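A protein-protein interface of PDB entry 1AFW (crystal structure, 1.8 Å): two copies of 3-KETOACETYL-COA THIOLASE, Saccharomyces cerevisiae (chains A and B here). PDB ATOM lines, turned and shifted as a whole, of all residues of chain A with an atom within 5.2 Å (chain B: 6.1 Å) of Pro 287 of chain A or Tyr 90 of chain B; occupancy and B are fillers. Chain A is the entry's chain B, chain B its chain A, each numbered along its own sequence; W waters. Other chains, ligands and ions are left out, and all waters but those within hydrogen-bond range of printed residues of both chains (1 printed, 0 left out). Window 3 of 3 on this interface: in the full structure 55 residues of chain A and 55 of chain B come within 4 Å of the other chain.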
ATOM      1  N   GLY A 285     -13.262  -2.615 -10.449  1.00  0.00           N
ATOM      2  CA  GLY A 285     -14.633  -2.417  -9.975  1.00  0.00           C
ATOM      3  C   GLY A 285     -15.580  -2.381 -11.236  1.00  0.00           C
ATOM      4  O   GLY A 285     -15.200  -1.943 -12.340  1.00  0.00           O
ATOM      5  N   VAL A 286     -16.819  -2.850 -11.090  1.00  0.00           N
ATOM      6  CA  VAL A 286     -17.789  -2.823 -12.199  1.00  0.00           C
ATOM      7  C   VAL A 286     -19.105  -2.413 -11.488  1.00  0.00           C
ATOM      8  O   VAL A 286     -19.199  -2.529 -10.216  1.00  0.00           O
ATOM      9  CB  VAL A 286     -17.944  -4.205 -12.887  1.00  0.00           C
ATOM     10  CG1 VAL A 286     -16.618  -4.738 -13.498  1.00  0.00           C
ATOM     11  CG2 VAL A 286     -18.511  -5.287 -11.970  1.00  0.00           C
ATOM     12  N   PRO A 287     -20.100  -1.943 -12.258  1.00  0.00           N
ATOM     13  CA  PRO A 287     -21.404  -1.500 -11.659  1.00  0.00           C
ATOM     14  C   PRO A 287     -21.943  -2.600 -10.741  1.00  0.00           C
ATOM     15  O   PRO A 287     -21.992  -3.786 -11.167  1.00  0.00           O
ATOM     16  CB  PRO A 287     -22.303  -1.299 -12.887  1.00  0.00           C
ATOM     17  CG  PRO A 287     -21.336  -1.047 -14.007  1.00  0.00           C
ATOM     18  CD  PRO A 287     -20.151  -1.961 -13.747  1.00  0.00           C
ATOM     19  N   PRO A 288     -22.298  -2.272  -9.494  1.00  0.00           N
ATOM     20  CA  PRO A 288     -22.768  -3.336  -8.587  1.00  0.00           C
ATOM     21  C   PRO A 288     -24.003  -4.084  -9.108  1.00  0.00           C
ATOM     22  O   PRO A 288     -24.228  -5.268  -8.758  1.00  0.00           O
ATOM     23  CB  PRO A 288     -23.150  -2.575  -7.304  1.00  0.00           C
ATOM     24  CG  PRO A 288     -22.186  -1.523  -7.305  1.00  0.00           C
ATOM     25  CD  PRO A 288     -22.154  -1.020  -8.757  1.00  0.00           C
ATOM     26  N   GLU A 289     -24.797  -3.354  -9.907  1.00  0.00           N
ATOM     27  CA  GLU A 289     -26.057  -3.889 -10.456  1.00  0.00           C
ATOM     28  C   GLU A 289     -25.910  -5.024 -11.405  1.00  0.00           C
ATOM     29  O   GLU A 289     -26.860  -5.759 -11.639  1.00  0.00           O
ATOM     30  CB  GLU A 289     -27.063  -2.816 -10.906  1.00  0.00           C
ATOM     31  CG  GLU A 289     -26.560  -1.969 -11.995  1.00  0.00           C
ATOM     32  CD  GLU A 289     -25.829  -0.728 -11.500  1.00  0.00           C
ATOM     33  OE1 GLU A 289     -24.838  -0.874 -10.726  1.00  0.00           O
ATOM     34  OE2 GLU A 289     -26.226   0.394 -11.919  1.00  0.00           O
ATOM     35  N   ILE A 290     -24.714  -5.170 -11.951  1.00  0.00           N
ATOM     36  CA  ILE A 290     -24.405  -6.261 -12.872  1.00  0.00           C
ATOM     37  C   ILE A 290     -23.002  -6.783 -12.482  1.00  0.00           C
ATOM     38  O   ILE A 290     -22.143  -6.999 -13.336  1.00  0.00           O
ATOM     39  CB  ILE A 290     -24.420  -5.758 -14.396  1.00  0.00           C
ATOM     40  CG1 ILE A 290     -23.488  -4.554 -14.584  1.00  0.00           C
ATOM     41  CG2 ILE A 290     -25.914  -5.445 -14.835  1.00  0.00           C
ATOM     42  CD1 ILE A 290     -23.272  -4.229 -16.108  1.00  0.00           C
ATOM     43  N   MET A 291     -22.775  -6.990 -11.184  1.00  0.00           N
ATOM     44  CA  MET A 291     -21.478  -7.466 -10.646  1.00  0.00           C
ATOM     45  C   MET A 291     -20.938  -8.716 -11.330  1.00  0.00           C
ATOM     46  O   MET A 291     -19.737  -8.932 -11.355  1.00  0.00           O
ATOM     47  CB  MET A 291     -21.557  -7.751  -9.132  1.00  0.00           C
ATOM     48  CG  MET A 291     -22.488  -8.898  -8.809  1.00  0.00           C
ATOM     49  SD  MET A 291     -21.533 -10.355  -8.592  1.00  0.00           S
ATOM     50  CE  MET A 291     -22.651 -11.690  -8.906  1.00  0.00           C
ATOM     51  N   VAL A 293     -20.401  -9.309 -14.297  1.00  0.00           N
ATOM     52  CA  VAL A 293     -19.517  -9.117 -15.438  1.00  0.00           C
ATOM     53  C   VAL A 293     -18.033  -8.938 -14.967  1.00  0.00           C
ATOM     54  O   VAL A 293     -17.172  -8.707 -15.817  1.00  0.00           O
ATOM     55  CB  VAL A 293     -19.869  -7.788 -16.136  1.00  0.00           C
ATOM     56  CG1 VAL A 293     -21.313  -7.789 -16.792  1.00  0.00           C
ATOM     57  CG2 VAL A 293     -19.818  -6.634 -15.164  1.00  0.00           C
ATOM     58  N   GLY A 383     -19.950  -5.248  -6.795  1.00  0.00           N
ATOM     59  CA  GLY A 383     -19.373  -4.821  -8.062  1.00  0.00           C
ATOM     60  C   GLY A 383     -17.887  -4.823  -8.324  1.00  0.00           C
ATOM     61  O   GLY A 383     -17.322  -3.738  -8.498  1.00  0.00           O
ATOM     62  N   ARG B  80     -18.142  -0.281   1.297  1.00  0.00           N
ATOM     63  CA  ARG B  80     -18.002  -0.095  -0.140  1.00  0.00           C
ATOM     64  C   ARG B  80     -19.211   0.819  -0.510  1.00  0.00           C
ATOM     65  O   ARG B  80     -19.061   1.712  -1.358  1.00  0.00           O
ATOM     66  CB  ARG B  80     -18.161  -1.505  -0.744  1.00  0.00           C
ATOM     67  CG  ARG B  80     -18.523  -1.666  -2.191  1.00  0.00           C
ATOM     68  CD  ARG B  80     -17.688  -0.882  -3.099  1.00  0.00           C
ATOM     69  NE  ARG B  80     -17.929  -1.361  -4.476  1.00  0.00           N
ATOM     70  CZ  ARG B  80     -17.264  -0.897  -5.531  1.00  0.00           C
ATOM     71  NH1 ARG B  80     -16.350   0.033  -5.353  1.00  0.00           N
ATOM     72  NH2 ARG B  80     -17.513  -1.320  -6.765  1.00  0.00           N
ATOM     73  N   LEU B  84     -19.037   4.464  -2.363  1.00  0.00           N
ATOM     74  CA  LEU B  84     -19.787   4.662  -3.607  1.00  0.00           C
ATOM     75  C   LEU B  84     -20.542   5.959  -3.500  1.00  0.00           C
ATOM     76  O   LEU B  84     -20.441   6.734  -4.451  1.00  0.00           O
ATOM     77  CB  LEU B  84     -20.814   3.561  -3.942  1.00  0.00           C
ATOM     78  CG  LEU B  84     -20.258   2.208  -4.312  1.00  0.00           C
ATOM     79  CD1 LEU B  84     -21.338   1.151  -4.402  1.00  0.00           C
ATOM     80  CD2 LEU B  84     -19.442   2.422  -5.582  1.00  0.00           C
ATOM     81  N   ILE B  88     -16.572   7.929  -4.869  1.00  0.00           N
ATOM     82  CA  ILE B  88     -15.392   7.164  -5.305  1.00  0.00           C
ATOM     83  C   ILE B  88     -16.087   6.233  -6.277  1.00  0.00           C
ATOM     84  O   ILE B  88     -16.996   5.512  -5.871  1.00  0.00           O
ATOM     85  CB  ILE B  88     -14.748   6.410  -4.106  1.00  0.00           C
ATOM     86  CG1 ILE B  88     -14.076   7.419  -3.169  1.00  0.00           C
ATOM     87  CG2 ILE B  88     -13.625   5.509  -4.667  1.00  0.00           C
ATOM     88  CD1 ILE B  88     -13.316   6.705  -2.065  1.00  0.00           C
ATOM     89  N   PRO B  89     -15.712   6.265  -7.547  1.00  0.00           N
ATOM     90  CA  PRO B  89     -16.384   5.438  -8.529  1.00  0.00           C
ATOM     91  C   PRO B  89     -16.415   3.921  -8.371  1.00  0.00           C
ATOM     92  O   PRO B  89     -15.521   3.338  -7.756  1.00  0.00           O
ATOM     93  CB  PRO B  89     -15.786   5.883  -9.871  1.00  0.00           C
ATOM     94  CG  PRO B  89     -14.500   6.520  -9.556  1.00  0.00           C
ATOM     95  CD  PRO B  89     -14.588   7.027  -8.129  1.00  0.00           C
ATOM     96  N   TYR B  90     -17.433   3.273  -8.942  1.00  0.00           N
ATOM     97  CA  TYR B  90     -17.507   1.835  -8.784  1.00  0.00           C
ATOM     98  C   TYR B  90     -16.300   1.160  -9.329  1.00  0.00           C
ATOM     99  O   TYR B  90     -15.974   0.019  -8.943  1.00  0.00           O
ATOM    100  CB  TYR B  90     -18.781   1.258  -9.390  1.00  0.00           C
ATOM    101  CG  TYR B  90     -18.832   1.483 -10.850  1.00  0.00           C
ATOM    102  CD1 TYR B  90     -18.081   0.688 -11.690  1.00  0.00           C
ATOM    103  CD2 TYR B  90     -19.652   2.468 -11.373  1.00  0.00           C
ATOM    104  CE1 TYR B  90     -18.076   0.882 -13.031  1.00  0.00           C
ATOM    105  CE2 TYR B  90     -19.702   2.668 -12.725  1.00  0.00           C
ATOM    106  CZ  TYR B  90     -18.908   1.880 -13.561  1.00  0.00           C
ATOM    107  OH  TYR B  90     -18.921   2.061 -14.943  1.00  0.00           O
ATOM    108  N   SER B  91     -15.665   1.850 -10.272  1.00  0.00           N
ATOM    109  CA  SER B  91     -14.504   1.223 -10.875  1.00  0.00           C
ATOM    110  C   SER B  91     -13.336   1.050  -9.921  1.00  0.00           C
ATOM    111  O   SER B  91     -12.420   0.338 -10.263  1.00  0.00           O
ATOM    112  CB  SER B  91     -14.029   1.937 -12.148  1.00  0.00           C
ATOM    113  OG  SER B  91     -13.709   3.274 -11.830  1.00  0.00           O
ATOM    114  N   THR B  92     -13.365   1.694  -8.759  1.00  0.00           N
ATOM    115  CA  THR B  92     -12.266   1.555  -7.780  1.00  0.00           C
ATOM    116  C   THR B  92     -12.619   0.377  -6.837  1.00  0.00           C
ATOM    117  O   THR B  92     -13.663   0.471  -6.196  1.00  0.00           O
ATOM    118  CB  THR B  92     -12.271   2.810  -6.886  1.00  0.00           C
ATOM    119  OG1 THR B  92     -11.874   3.960  -7.677  1.00  0.00           O
ATOM    120  CG2 THR B  92     -11.283   2.580  -5.756  1.00  0.00           C
ATOM    121  N   PRO B  93     -11.790  -0.667  -6.735  1.00  0.00           N
ATOM    122  CA  PRO B  93     -12.061  -1.828  -5.894  1.00  0.00           C
ATOM    123  C   PRO B  93     -11.982  -1.482  -4.428  1.00  0.00           C
ATOM    124  O   PRO B  93     -11.410  -0.452  -4.095  1.00  0.00           O
ATOM    125  CB  PRO B  93     -11.025  -2.881  -6.300  1.00  0.00           C
ATOM    126  CG  PRO B  93     -10.406  -2.398  -7.485  1.00  0.00           C
ATOM    127  CD  PRO B  93     -10.633  -0.917  -7.623  1.00  0.00           C
HETATM  128  O   HOH W   1     -11.555  -1.095 -12.323  1.00  0.00           O
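The guanidinium group of Arg 80 of chain B sits at hydrogen-bond distance from the backbone carbonyl oxygen of Gly 383 of chain A (3.0 Å). N of Gly 285 of chain A sits at hydrogen-bond distance from O of Ser 91 of chain B.
Pro 287 of chain A touches one residue of chain B. Of the printed residues of chain B, Val 286 of chain A touches Tyr 90 (3.3 Å). Printed residues of chain B within 4 Å of Gly 383 of chain A: Arg 80 (3.0 Å). Of the printed residues of chain A, Arg 80 of chain B touches Gly 383 (3.0 Å). Of the printed residues of chain A, Ser 91 of chain B touches Gly 285. Of the printed residues of chain B, Gly 285 of chain A touches Tyr 90 and Ser 91. Leu 84 of chain B touches none of the printed residues of chain A. The nearest printed residue of chain B that does not touch Pro 287 of chain A is Arg 80 of chain B (6.1 Å). The nearest printed residue of chain A that does not touch Tyr 90 of chain B is Gly 383 of chain A (4.02 Å).
No position is printed for both chains.
Printed residues of chain B that touch a printed residue of chain A: Arg 80, Tyr 90 and Ser 91. Hydrophobic or aromatic side chains of chain A that line the printed part of chain B: Pro 287. Among the printed residues, 5 pairs touch across the chains.
The guanidinium group (NH2) of Arg 80 of chain B sits at hydrogen-bond distance from the backbone carbonyl oxygen (O) of Tyr 90 of chain B. The guanidinium group (NH1) of Arg 80 of chain B is in hydrogen-bond range of the backbone carbonyl oxygen (O) of Thr 92 of chain B. N of Val 286 of chain A sits at hydrogen-bond distance from O of Gly 383 of chain A (2.8 Å).
Tyr 90 of chain B touches Gly 285 of chain A (O to CA, 3.0 Å). Tyr 90 of chain B touches Val 286 of chain A. Tyr 90 of chain B touches Pro 287 of chain A.
Water W1 lies within hydrogen-bond range of the backbone carbonyl oxygen (O) of Ser 91 of chain B (2.7 Å) and the backbone NH (N) of Gly 285 of chain A (3.0 Å).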
